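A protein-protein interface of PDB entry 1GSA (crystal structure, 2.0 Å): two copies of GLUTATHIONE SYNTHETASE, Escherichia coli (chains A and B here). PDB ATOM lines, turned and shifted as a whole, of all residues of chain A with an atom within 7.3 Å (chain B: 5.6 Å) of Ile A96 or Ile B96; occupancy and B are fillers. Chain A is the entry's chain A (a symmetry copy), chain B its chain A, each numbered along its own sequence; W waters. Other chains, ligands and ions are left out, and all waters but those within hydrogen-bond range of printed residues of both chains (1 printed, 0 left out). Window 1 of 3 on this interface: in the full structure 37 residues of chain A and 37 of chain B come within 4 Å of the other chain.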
ATOM      1  N   MET A  40      13.153   6.445  16.551  1.00  0.00           N
ATOM      2  CA  MET A  40      12.207   6.025  17.585  1.00  0.00           C
ATOM      3  C   MET A  40      11.057   6.984  17.800  1.00  0.00           C
ATOM      4  O   MET A  40       9.955   6.567  18.031  1.00  0.00           O
ATOM      5  CB  MET A  40      12.907   5.855  18.934  1.00  0.00           C
ATOM      6  CG  MET A  40      13.963   4.784  18.959  1.00  0.00           C
ATOM      7  SD  MET A  40      13.245   3.185  19.312  1.00  0.00           S
ATOM      8  CE  MET A  40      13.240   3.433  21.064  1.00  0.00           C
ATOM      9  N   MET A  85      14.772  -3.443  12.562  1.00  0.00           N
ATOM     10  CA  MET A  85      14.892  -2.776  13.830  1.00  0.00           C
ATOM     11  C   MET A  85      16.389  -2.757  14.144  1.00  0.00           C
ATOM     12  O   MET A  85      17.012  -3.727  14.572  1.00  0.00           O
ATOM     13  CB  MET A  85      14.065  -3.557  14.851  1.00  0.00           C
ATOM     14  CG  MET A  85      14.164  -3.017  16.271  1.00  0.00           C
ATOM     15  SD  MET A  85      13.959  -1.226  16.315  1.00  0.00           S
ATOM     16  CE  MET A  85      13.353  -0.928  17.927  1.00  0.00           C
ATOM     17  N   PRO A  90      21.421   0.866  24.925  1.00  0.00           N
ATOM     18  CA  PRO A  90      20.820  -0.048  25.876  1.00  0.00           C
ATOM     19  C   PRO A  90      19.425  -0.563  25.693  1.00  0.00           C
ATOM     20  O   PRO A  90      18.568  -0.045  24.980  1.00  0.00           O
ATOM     21  CB  PRO A  90      20.973   0.643  27.199  1.00  0.00           C
ATOM     22  CG  PRO A  90      21.020   2.090  26.855  1.00  0.00           C
ATOM     23  CD  PRO A  90      21.920   2.042  25.626  1.00  0.00           C
ATOM     24  N   PHE A  91      19.292  -1.722  26.293  1.00  0.00           N
ATOM     25  CA  PHE A  91      18.039  -2.420  26.391  1.00  0.00           C
ATOM     26  C   PHE A  91      17.363  -1.707  27.549  1.00  0.00           C
ATOM     27  O   PHE A  91      17.757  -1.832  28.709  1.00  0.00           O
ATOM     28  CB  PHE A  91      18.373  -3.842  26.706  1.00  0.00           C
ATOM     29  CG  PHE A  91      17.199  -4.738  27.017  1.00  0.00           C
ATOM     30  CD1 PHE A  91      16.416  -5.237  25.957  1.00  0.00           C
ATOM     31  CD2 PHE A  91      16.943  -5.073  28.360  1.00  0.00           C
ATOM     32  CE1 PHE A  91      15.358  -6.099  26.259  1.00  0.00           C
ATOM     33  CE2 PHE A  91      15.879  -5.936  28.635  1.00  0.00           C
ATOM     34  CZ  PHE A  91      15.090  -6.449  27.598  1.00  0.00           C
ATOM     35  N   ASP A  92      16.411  -0.871  27.249  1.00  0.00           N
ATOM     36  CA  ASP A  92      15.742  -0.160  28.296  1.00  0.00           C
ATOM     37  C   ASP A  92      14.271  -0.340  28.029  1.00  0.00           C
ATOM     38  O   ASP A  92      13.919  -0.985  27.036  1.00  0.00           O
ATOM     39  CB  ASP A  92      16.178   1.311  28.243  1.00  0.00           C
ATOM     40  CG  ASP A  92      16.088   2.047  26.921  1.00  0.00           C
ATOM     41  OD1 ASP A  92      15.422   1.608  25.997  1.00  0.00           O
ATOM     42  OD2 ASP A  92      16.706   3.091  26.808  1.00  0.00           O
ATOM     43  N   THR A  93      13.402   0.264  28.828  1.00  0.00           N
ATOM     44  CA  THR A  93      11.966   0.137  28.620  1.00  0.00           C
ATOM     45  C   THR A  93      11.522   0.851  27.365  1.00  0.00           C
ATOM     46  O   THR A  93      10.606   0.352  26.737  1.00  0.00           O
ATOM     47  CB  THR A  93      11.175   0.685  29.807  1.00  0.00           C
ATOM     48  OG1 THR A  93      11.911   1.748  30.388  1.00  0.00           O
ATOM     49  CG2 THR A  93      10.930  -0.392  30.838  1.00  0.00           C
ATOM     50  N   GLU A  94      12.133   1.953  26.909  1.00  0.00           N
ATOM     51  CA  GLU A  94      11.794   2.586  25.650  1.00  0.00           C
ATOM     52  C   GLU A  94      11.927   1.639  24.474  1.00  0.00           C
ATOM     53  O   GLU A  94      11.051   1.536  23.613  1.00  0.00           O
ATOM     54  CB  GLU A  94      12.684   3.775  25.481  1.00  0.00           C
ATOM     55  CG  GLU A  94      12.341   4.900  26.451  1.00  0.00           C
ATOM     56  CD  GLU A  94      10.880   5.271  26.348  1.00  0.00           C
ATOM     57  OE1 GLU A  94      10.449   5.718  25.276  1.00  0.00           O
ATOM     58  OE2 GLU A  94      10.170   5.093  27.335  1.00  0.00           O
ATOM     59  N   PHE A  95      13.023   0.869  24.493  1.00  0.00           N
ATOM     60  CA  PHE A  95      13.277  -0.155  23.498  1.00  0.00           C
ATOM     61  C   PHE A  95      12.128  -1.176  23.515  1.00  0.00           C
ATOM     62  O   PHE A  95      11.572  -1.488  22.462  1.00  0.00           O
ATOM     63  CB  PHE A  95      14.611  -0.823  23.822  1.00  0.00           C
ATOM     64  CG  PHE A  95      15.099  -1.650  22.650  1.00  0.00           C
ATOM     65  CD1 PHE A  95      14.675  -2.969  22.486  1.00  0.00           C
ATOM     66  CD2 PHE A  95      15.928  -1.056  21.714  1.00  0.00           C
ATOM     67  CE1 PHE A  95      15.073  -3.695  21.368  1.00  0.00           C
ATOM     68  CE2 PHE A  95      16.323  -1.782  20.600  1.00  0.00           C
ATOM     69  CZ  PHE A  95      15.891  -3.099  20.429  1.00  0.00           C
ATOM     70  N   ILE A  96      11.723  -1.647  24.709  1.00  0.00           N
ATOM     71  CA  ILE A  96      10.613  -2.564  24.856  1.00  0.00           C
ATOM     72  C   ILE A  96       9.347  -1.940  24.348  1.00  0.00           C
ATOM     73  O   ILE A  96       8.646  -2.593  23.588  1.00  0.00           O
ATOM     74  CB  ILE A  96      10.497  -2.965  26.340  1.00  0.00           C
ATOM     75  CG1 ILE A  96      11.568  -4.006  26.491  1.00  0.00           C
ATOM     76  CG2 ILE A  96       9.203  -3.607  26.776  1.00  0.00           C
ATOM     77  CD1 ILE A  96      12.103  -3.976  27.889  1.00  0.00           C
ATOM     78  N   TYR A  97       9.017  -0.688  24.652  1.00  0.00           N
ATOM     79  CA  TYR A  97       7.776  -0.086  24.175  1.00  0.00           C
ATOM     80  C   TYR A  97       7.792  -0.036  22.662  1.00  0.00           C
ATOM     81  O   TYR A  97       6.777  -0.363  22.051  1.00  0.00           O
ATOM     82  CB  TYR A  97       7.600   1.335  24.735  1.00  0.00           C
ATOM     83  CG  TYR A  97       7.537   1.397  26.248  1.00  0.00           C
ATOM     84  CD1 TYR A  97       6.997   0.349  27.011  1.00  0.00           C
ATOM     85  CD2 TYR A  97       8.047   2.524  26.879  1.00  0.00           C
ATOM     86  CE1 TYR A  97       6.969   0.438  28.404  1.00  0.00           C
ATOM     87  CE2 TYR A  97       8.027   2.606  28.264  1.00  0.00           C
ATOM     88  CZ  TYR A  97       7.489   1.568  29.009  1.00  0.00           C
ATOM     89  OH  TYR A  97       7.463   1.686  30.380  1.00  0.00           O
ATOM     90  N   ALA A  98       8.911   0.277  22.015  1.00  0.00           N
ATOM     91  CA  ALA A  98       8.963   0.254  20.583  1.00  0.00           C
ATOM     92  C   ALA A  98       8.664  -1.128  20.035  1.00  0.00           C
ATOM     93  O   ALA A  98       7.999  -1.240  18.997  1.00  0.00           O
ATOM     94  CB  ALA A  98      10.335   0.699  20.155  1.00  0.00           C
ATOM     95  N   THR A  99       8.996  -2.235  20.703  1.00  0.00           N
ATOM     96  CA  THR A  99       8.741  -3.542  20.121  1.00  0.00           C
ATOM     97  C   THR A  99       7.255  -3.850  20.125  1.00  0.00           C
ATOM     98  O   THR A  99       6.801  -4.648  19.294  1.00  0.00           O
ATOM     99  CB  THR A  99       9.517  -4.671  20.875  1.00  0.00           C
ATOM    100  OG1 THR A  99       8.969  -4.759  22.169  1.00  0.00           O
ATOM    101  CG2 THR A  99      11.038  -4.394  21.022  1.00  0.00           C
ATOM    102  N   TYR A 100       6.420  -3.227  20.977  1.00  0.00           N
ATOM    103  CA  TYR A 100       4.975  -3.489  20.963  1.00  0.00           C
ATOM    104  C   TYR A 100       4.357  -2.777  19.785  1.00  0.00           C
ATOM    105  O   TYR A 100       3.397  -3.268  19.204  1.00  0.00           O
ATOM    106  CB  TYR A 100       4.240  -2.976  22.181  1.00  0.00           C
ATOM    107  CG  TYR A 100       4.707  -3.561  23.480  1.00  0.00           C
ATOM    108  CD1 TYR A 100       4.775  -4.931  23.675  1.00  0.00           C
ATOM    109  CD2 TYR A 100       5.036  -2.700  24.517  1.00  0.00           C
ATOM    110  CE1 TYR A 100       5.161  -5.433  24.916  1.00  0.00           C
ATOM    111  CE2 TYR A 100       5.429  -3.192  25.753  1.00  0.00           C
ATOM    112  CZ  TYR A 100       5.480  -4.560  25.936  1.00  0.00           C
ATOM    113  OH  TYR A 100       5.793  -5.048  27.174  1.00  0.00           O
ATOM    114  N   ILE A 101       4.904  -1.613  19.441  1.00  0.00           N
ATOM    115  CA  ILE A 101       4.488  -0.834  18.281  1.00  0.00           C
ATOM    116  C   ILE A 101       4.899  -1.623  17.063  1.00  0.00           C
ATOM    117  O   ILE A 101       4.082  -1.848  16.171  1.00  0.00           O
ATOM    118  CB  ILE A 101       5.157   0.549  18.308  1.00  0.00           C
ATOM    119  CG1 ILE A 101       4.600   1.302  19.503  1.00  0.00           C
ATOM    120  CG2 ILE A 101       4.967   1.266  16.980  1.00  0.00           C
ATOM    121  CD1 ILE A 101       5.411   2.550  19.807  1.00  0.00           C
ATOM    122  N   LEU A 102       6.115  -2.143  16.982  1.00  0.00           N
ATOM    123  CA  LEU A 102       6.474  -2.926  15.825  1.00  0.00           C
ATOM    124  C   LEU A 102       5.657  -4.198  15.765  1.00  0.00           C
ATOM    125  O   LEU A 102       5.296  -4.685  14.695  1.00  0.00           O
ATOM    126  CB  LEU A 102       7.926  -3.176  15.922  1.00  0.00           C
ATOM    127  CG  LEU A 102       8.756  -1.910  15.742  1.00  0.00           C
ATOM    128  CD1 LEU A 102      10.212  -2.217  15.997  1.00  0.00           C
ATOM    129  CD2 LEU A 102       8.609  -1.393  14.340  1.00  0.00           C
ATOM    130  N   PRO A 116       9.864  -8.875  17.263  1.00  0.00           N
ATOM    131  CA  PRO A 116       9.693  -8.081  18.474  1.00  0.00           C
ATOM    132  C   PRO A 116       9.551  -8.934  19.714  1.00  0.00           C
ATOM    133  O   PRO A 116      10.135  -8.638  20.755  1.00  0.00           O
ATOM    134  CB  PRO A 116       8.474  -7.248  18.195  1.00  0.00           C
ATOM    135  CG  PRO A 116       8.459  -7.119  16.712  1.00  0.00           C
ATOM    136  CD  PRO A 116       8.791  -8.538  16.317  1.00  0.00           C
ATOM    137  N   LEU A 119      12.965 -10.133  20.652  1.00  0.00           N
ATOM    138  CA  LEU A 119      13.833  -9.088  21.191  1.00  0.00           C
ATOM    139  C   LEU A 119      13.614  -8.840  22.664  1.00  0.00           C
ATOM    140  O   LEU A 119      14.517  -8.402  23.366  1.00  0.00           O
ATOM    141  CB  LEU A 119      13.612  -7.777  20.459  1.00  0.00           C
ATOM    142  CG  LEU A 119      14.015  -7.763  19.003  1.00  0.00           C
ATOM    143  CD1 LEU A 119      13.620  -6.453  18.371  1.00  0.00           C
ATOM    144  CD2 LEU A 119      15.508  -7.910  18.896  1.00  0.00           C
ATOM    145  N   ARG A 120      12.403  -9.082  23.133  1.00  0.00           N
ATOM    146  CA  ARG A 120      12.065  -8.992  24.542  1.00  0.00           C
ATOM    147  C   ARG A 120      12.382 -10.281  25.270  1.00  0.00           C
ATOM    148  O   ARG A 120      12.571 -10.245  26.469  1.00  0.00           O
ATOM    149  CB  ARG A 120      10.569  -8.718  24.760  1.00  0.00           C
ATOM    150  CG  ARG A 120      10.050  -7.432  24.199  1.00  0.00           C
ATOM    151  CD  ARG A 120       8.613  -7.153  24.669  1.00  0.00           C
ATOM    152  NE  ARG A 120       7.656  -8.154  24.219  1.00  0.00           N
ATOM    153  CZ  ARG A 120       6.931  -8.027  23.106  1.00  0.00           C
ATOM    154  NH1 ARG A 120       7.020  -6.976  22.300  1.00  0.00           N
ATOM    155  NH2 ARG A 120       6.031  -8.962  22.853  1.00  0.00           N
ATOM    156  N   ASP A 121      12.348 -11.444  24.628  1.00  0.00           N
ATOM    157  CA  ASP A 121      12.676 -12.711  25.260  1.00  0.00           C
ATOM    158  C   ASP A 121      14.170 -12.939  25.343  1.00  0.00           C
ATOM    159  O   ASP A 121      14.655 -13.535  26.304  1.00  0.00           O
ATOM    160  CB  ASP A 121      12.147 -13.924  24.498  1.00  0.00           C
ATOM    161  CG  ASP A 121      10.641 -14.102  24.377  1.00  0.00           C
ATOM    162  OD1 ASP A 121       9.862 -13.565  25.151  1.00  0.00           O
ATOM    163  OD2 ASP A 121      10.237 -14.791  23.466  1.00  0.00           O
ATOM    164  N   ASN A 123      17.474 -11.383  25.809  1.00  0.00           N
ATOM    165  CA  ASN A 123      18.385 -10.336  26.214  1.00  0.00           C
ATOM    166  C   ASN A 123      19.781 -10.808  25.817  1.00  0.00           C
ATOM    167  O   ASN A 123      20.088 -11.992  25.985  1.00  0.00           O
ATOM    168  CB  ASN A 123      18.261 -10.164  27.688  1.00  0.00           C
ATOM    169  CG  ASN A 123      19.377  -9.340  28.281  1.00  0.00           C
ATOM    170  OD1 ASN A 123      20.317  -9.905  28.818  1.00  0.00           O
ATOM    171  ND2 ASN A 123      19.449  -8.028  28.190  1.00  0.00           N
ATOM    172  N   LEU A 126      21.458 -12.473  29.003  1.00  0.00           N
ATOM    173  CA  LEU A 126      20.789 -13.579  29.679  1.00  0.00           C
ATOM    174  C   LEU A 126      20.263 -14.706  28.819  1.00  0.00           C
ATOM    175  O   LEU A 126      19.951 -15.789  29.326  1.00  0.00           O
ATOM    176  CB  LEU A 126      19.654 -13.036  30.534  1.00  0.00           C
ATOM    177  CG  LEU A 126      20.106 -12.069  31.620  1.00  0.00           C
ATOM    178  CD1 LEU A 126      18.954 -11.669  32.498  1.00  0.00           C
ATOM    179  CD2 LEU A 126      21.124 -12.736  32.500  1.00  0.00           C
ATOM    180  N   TYR A 194      20.722  -6.552  39.412  1.00  0.00           N
ATOM    181  CA  TYR A 194      21.432  -7.783  39.055  1.00  0.00           C
ATOM    182  C   TYR A 194      22.649  -7.447  38.215  1.00  0.00           C
ATOM    183  O   TYR A 194      22.589  -6.481  37.447  1.00  0.00           O
ATOM    184  CB  TYR A 194      20.589  -8.749  38.187  1.00  0.00           C
ATOM    185  CG  TYR A 194      19.332  -9.325  38.816  1.00  0.00           C
ATOM    186  CD1 TYR A 194      19.404 -10.225  39.879  1.00  0.00           C
ATOM    187  CD2 TYR A 194      18.091  -8.887  38.369  1.00  0.00           C
ATOM    188  CE1 TYR A 194      18.233 -10.671  40.509  1.00  0.00           C
ATOM    189  CE2 TYR A 194      16.925  -9.328  38.995  1.00  0.00           C
ATOM    190  CZ  TYR A 194      17.000 -10.213  40.069  1.00  0.00           C
ATOM    191  OH  TYR A 194      15.849 -10.576  40.720  1.00  0.00           O
ATOM    192  N   PHE B  91       7.433  -1.142  36.032  1.00  0.00           N
ATOM    193  CA  PHE B  91       7.852  -2.068  35.014  1.00  0.00           C
ATOM    194  C   PHE B  91       9.191  -1.491  34.587  1.00  0.00           C
ATOM    195  O   PHE B  91       9.272  -0.440  33.950  1.00  0.00           O
ATOM    196  CB  PHE B  91       6.823  -1.999  33.933  1.00  0.00           C
ATOM    197  CG  PHE B  91       7.140  -2.774  32.677  1.00  0.00           C
ATOM    198  CD1 PHE B  91       6.949  -4.170  32.665  1.00  0.00           C
ATOM    199  CD2 PHE B  91       7.585  -2.068  31.544  1.00  0.00           C
ATOM    200  CE1 PHE B  91       7.206  -4.868  31.480  1.00  0.00           C
ATOM    201  CE2 PHE B  91       7.836  -2.789  30.373  1.00  0.00           C
ATOM    202  CZ  PHE B  91       7.649  -4.176  30.335  1.00  0.00           C
ATOM    203  N   ASP B  92      10.257  -2.104  35.013  1.00  0.00           N
ATOM    204  CA  ASP B  92      11.548  -1.603  34.652  1.00  0.00           C
ATOM    205  C   ASP B  92      12.315  -2.795  34.143  1.00  0.00           C
ATOM    206  O   ASP B  92      11.767  -3.903  34.144  1.00  0.00           O
ATOM    207  CB  ASP B  92      12.193  -0.971  35.894  1.00  0.00           C
ATOM    208  CG  ASP B  92      12.245  -1.781  37.175  1.00  0.00           C
ATOM    209  OD1 ASP B  92      12.065  -2.989  37.167  1.00  0.00           O
ATOM    210  OD2 ASP B  92      12.469  -1.187  38.215  1.00  0.00           O
ATOM    211  N   THR B  93      13.580  -2.628  33.779  1.00  0.00           N
ATOM    212  CA  THR B  93      14.379  -3.742  33.285  1.00  0.00           C
ATOM    213  C   THR B  93      14.677  -4.740  34.380  1.00  0.00           C
ATOM    214  O   THR B  93      14.734  -5.913  34.061  1.00  0.00           O
ATOM    215  CB  THR B  93      15.697  -3.263  32.679  1.00  0.00           C
ATOM    216  OG1 THR B  93      16.108  -2.092  33.362  1.00  0.00           O
ATOM    217  CG2 THR B  93      15.541  -2.968  31.206  1.00  0.00           C
ATOM    218  N   GLU B  94      14.817  -4.379  35.664  1.00  0.00           N
ATOM    219  CA  GLU B  94      14.992  -5.332  36.741  1.00  0.00           C
ATOM    220  C   GLU B  94      13.858  -6.335  36.815  1.00  0.00           C
ATOM    221  O   GLU B  94      14.059  -7.546  36.932  1.00  0.00           O
ATOM    222  CB  GLU B  94      15.107  -4.564  38.018  1.00  0.00           C
ATOM    223  CG  GLU B  94      16.421  -3.797  38.118  1.00  0.00           C
ATOM    224  CD  GLU B  94      17.598  -4.721  37.908  1.00  0.00           C
ATOM    225  OE1 GLU B  94      17.783  -5.649  38.709  1.00  0.00           O
ATOM    226  OE2 GLU B  94      18.319  -4.524  36.932  1.00  0.00           O
ATOM    227  N   PHE B  95      12.634  -5.813  36.654  1.00  0.00           N
ATOM    228  CA  PHE B  95      11.436  -6.628  36.609  1.00  0.00           C
ATOM    229  C   PHE B  95      11.546  -7.629  35.447  1.00  0.00           C
ATOM    230  O   PHE B  95      11.328  -8.825  35.648  1.00  0.00           O
ATOM    231  CB  PHE B  95      10.231  -5.707  36.428  1.00  0.00           C
ATOM    232  CG  PHE B  95       8.940  -6.445  36.715  1.00  0.00           C
ATOM    233  CD1 PHE B  95       8.307  -7.184  35.714  1.00  0.00           C
ATOM    234  CD2 PHE B  95       8.428  -6.420  38.001  1.00  0.00           C
ATOM    235  CE1 PHE B  95       7.161  -7.915  36.007  1.00  0.00           C
ATOM    236  CE2 PHE B  95       7.286  -7.150  38.291  1.00  0.00           C
ATOM    237  CZ  PHE B  95       6.657  -7.898  37.293  1.00  0.00           C
ATOM    238  N   ILE B  96      11.948  -7.163  34.252  1.00  0.00           N
ATOM    239  CA  ILE B  96      12.148  -8.018  33.101  1.00  0.00           C
ATOM    240  C   ILE B  96      13.210  -9.039  33.385  1.00  0.00           C
ATOM    241  O   ILE B  96      12.976 -10.207  33.114  1.00  0.00           O
ATOM    242  CB  ILE B  96      12.510  -7.138  31.888  1.00  0.00           C
ATOM    243  CG1 ILE B  96      11.176  -6.609  31.448  1.00  0.00           C
ATOM    244  CG2 ILE B  96      13.117  -7.834  30.694  1.00  0.00           C
ATOM    245  CD1 ILE B  96      11.352  -5.256  30.833  1.00  0.00           C
ATOM    246  N   TYR B  97      14.354  -8.706  33.977  1.00  0.00           N
ATOM    247  CA  TYR B  97      15.398  -9.694  34.236  1.00  0.00           C
ATOM    248  C   TYR B  97      14.864 -10.751  35.179  1.00  0.00           C
ATOM    249  O   TYR B  97      15.105 -11.931  34.937  1.00  0.00           O
ATOM    250  CB  TYR B  97      16.642  -9.034  34.853  1.00  0.00           C
ATOM    251  CG  TYR B  97      17.279  -7.978  33.974  1.00  0.00           C
ATOM    252  CD1 TYR B  97      17.240  -8.058  32.571  1.00  0.00           C
ATOM    253  CD2 TYR B  97      17.902  -6.900  34.589  1.00  0.00           C
ATOM    254  CE1 TYR B  97      17.827  -7.057  31.796  1.00  0.00           C
ATOM    255  CE2 TYR B  97      18.476  -5.902  33.816  1.00  0.00           C
ATOM    256  CZ  TYR B  97      18.435  -5.992  32.433  1.00  0.00           C
ATOM    257  OH  TYR B  97      19.033  -4.999  31.691  1.00  0.00           O
ATOM    258  N   ALA B  98      14.083 -10.406  36.198  1.00  0.00           N
ATOM    259  CA  ALA B  98      13.508 -11.401  37.055  1.00  0.00           C
ATOM    260  C   ALA B  98      12.610 -12.350  36.284  1.00  0.00           C
ATOM    261  O   ALA B  98      12.600 -13.551  36.577  1.00  0.00           O
ATOM    262  CB  ALA B  98      12.725 -10.699  38.131  1.00  0.00           C
ATOM    263  N   THR B  99      11.916 -11.948  35.217  1.00  0.00           N
ATOM    264  CA  THR B  99      11.024 -12.872  34.536  1.00  0.00           C
ATOM    265  C   THR B  99      11.818 -13.913  33.768  1.00  0.00           C
ATOM    266  O   THR B  99      11.298 -15.011  33.527  1.00  0.00           O
ATOM    267  CB  THR B  99      10.052 -12.127  33.565  1.00  0.00           C
ATOM    268  OG1 THR B  99      10.834 -11.581  32.530  1.00  0.00           O
ATOM    269  CG2 THR B  99       9.271 -10.962  34.233  1.00  0.00           C
ATOM    270  N   TYR B 100      13.091 -13.683  33.399  1.00  0.00           N
ATOM    271  CA  TYR B 100      13.880 -14.698  32.690  1.00  0.00           C
ATOM    272  C   TYR B 100      14.322 -15.754  33.674  1.00  0.00           C
ATOM    273  O   TYR B 100      14.431 -16.921  33.317  1.00  0.00           O
ATOM    274  CB  TYR B 100      15.150 -14.170  32.062  1.00  0.00           C
ATOM    275  CG  TYR B 100      14.936 -13.093  31.041  1.00  0.00           C
ATOM    276  CD1 TYR B 100      14.073 -13.269  29.971  1.00  0.00           C
ATOM    277  CD2 TYR B 100      15.655 -11.912  31.160  1.00  0.00           C
ATOM    278  CE1 TYR B 100      13.946 -12.263  29.015  1.00  0.00           C
ATOM    279  CE2 TYR B 100      15.528 -10.904  30.216  1.00  0.00           C
ATOM    280  CZ  TYR B 100      14.674 -11.100  29.148  1.00  0.00           C
ATOM    281  OH  TYR B 100      14.603 -10.139  28.177  1.00  0.00           O
ATOM    282  N   ARG B 120       6.096  -9.801  30.127  1.00  0.00           N
ATOM    283  CA  ARG B 120       6.896  -8.990  29.229  1.00  0.00           C
ATOM    284  C   ARG B 120       6.117  -8.602  27.991  1.00  0.00           C
ATOM    285  O   ARG B 120       6.454  -7.613  27.371  1.00  0.00           O
ATOM    286  CB  ARG B 120       8.151  -9.731  28.745  1.00  0.00           C
ATOM    287  CG  ARG B 120       9.126 -10.131  29.807  1.00  0.00           C
ATOM    288  CD  ARG B 120      10.438 -10.653  29.200  1.00  0.00           C
ATOM    289  NE  ARG B 120      10.262 -11.859  28.401  1.00  0.00           N
ATOM    290  CZ  ARG B 120      10.419 -13.092  28.890  1.00  0.00           C
ATOM    291  NH1 ARG B 120      10.745 -13.333  30.153  1.00  0.00           N
ATOM    292  NH2 ARG B 120      10.320 -14.100  28.042  1.00  0.00           N
HETATM  293  O   HOH W   1      21.072  -4.813  36.271  1.00  0.00           O
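The backbone NH (N) of Tyr A194 sits at hydrogen-bond distance from the side-chain carboxylate (OE1) of Glu B94 (3.2 Å).
OH of Tyr B100 lies within hydrogen-bond range of O of Arg A120 (2.7 Å).
The side-chain hydroxyl of Tyr A100 is in hydrogen-bond range of the backbone carbonyl oxygen of Arg B120, 2.7 Å away.
NE of Arg B120 lies within hydrogen-bond range of O of Arg A120, 3.4 Å away.
The side-chain carboxylate (OD1) of Asp A121 is in salt-bridge range of the guanidinium group (NH2) of Arg B120, at 3.0 Å.
The side-chain hydroxyl (OG1) of Thr A99 is in hydrogen-bond range of the guanidinium group (NH1) of Arg A120.
The backbone NH (N) of Leu A126 is in hydrogen-bond range of the side-chain amide oxygen (OD1) of Asn A123 (2.8 Å).
O of Ile B96 is in hydrogen-bond range of OG1 of Thr B99 (2.6 Å).
The side-chain hydroxyl (OG1) of Thr B99 sits at hydrogen-bond distance from the guanidinium group (NH1) of Arg B120 (3.0 Å).
The side-chain hydroxyl (OG1) of Thr A99 sits at hydrogen-bond distance from the backbone carbonyl oxygen (O) of Ile A96, 2.6 Å away.
OD1 of Asp B92 sits close to N of Glu B94 (3.4 Å).
Among the printed residues, pairs that only touch across the chains: Phe A91 with Thr B93, Phe A91 with Ile B96, Phe A91 with Tyr B97, Phe A91 with Tyr B100, Thr A93 with Phe B91, Ile A96 with Phe B91, Ile A96 with Ile B96, Tyr A97 with Phe B91, Tyr A100 with Phe B91, Asp A121 with Tyr B100, Asn A123 with Tyr B100, Leu A126 with Tyr B97, Leu A126 with Tyr B100 and Tyr A194 with Tyr B97.
Of the printed residues of chain B, Phe A91 touches Thr B93 (3.5 Å), Ile B96 (3.9 Å), Tyr B97 (3.9 Å) and Tyr B100 (3.8 Å).
Of chain B, only Phe B91 (3.9 Å) and Ile B96 (3.3 Å) come within 4 Å of Ile A96.
Pro A116 touches none of the printed residues of chain B.
Printed residues of chain B within 4 Å of Arg A120: Tyr B100 and Arg B120.
Thr B99 touches none of the printed residues of chain A.
The nearest printed residue of chain B that does not touch Ile A96 is Thr B93 (4.9 Å).
The nearest printed residue of chain A that does not touch Ile B96 is Thr A93 (4.9 Å).
Of the 22 printed residues of chain A, 10 touch a printed residue of chain B.
Of the 11 printed residues of chain B, 7 touch a printed residue of chain A.
Hydrophobic or aromatic side chains of chain B within 4 Å of the printed part of chain A: Phe B91, Ile B96, Tyr B97 and Tyr B100.
Among the printed residues, 19 pairs touch across the chains.
Among the printed residues, Asp or Glu carboxylates within 4 Å of a Lys or Arg side-chain nitrogen of the other chain: Asp A121 with Arg B120.
Phe A91 touches Thr B93, and with the chains exchanged Thr A93 touches Phe B91.
Phe A91 touches Tyr B100, and with the chains exchanged Tyr A100 touches Phe B91.
Ile B96 touches its own counterpart, Ile A96.
Tyr A100 touches Arg B120, and with the chains exchanged Arg A120 touches Tyr B100.
Positions printed for both chains: 91, 92, 93, 94, 95, 96, 97, 98, 99, 100 and 120.
Of the 19 pairs that touch across the chains among the printed residues, 12 have their exchanged pair printed and touching as well.
Water W1 lies within hydrogen-bond range of O of Tyr A194 and OE2 of Glu B94.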
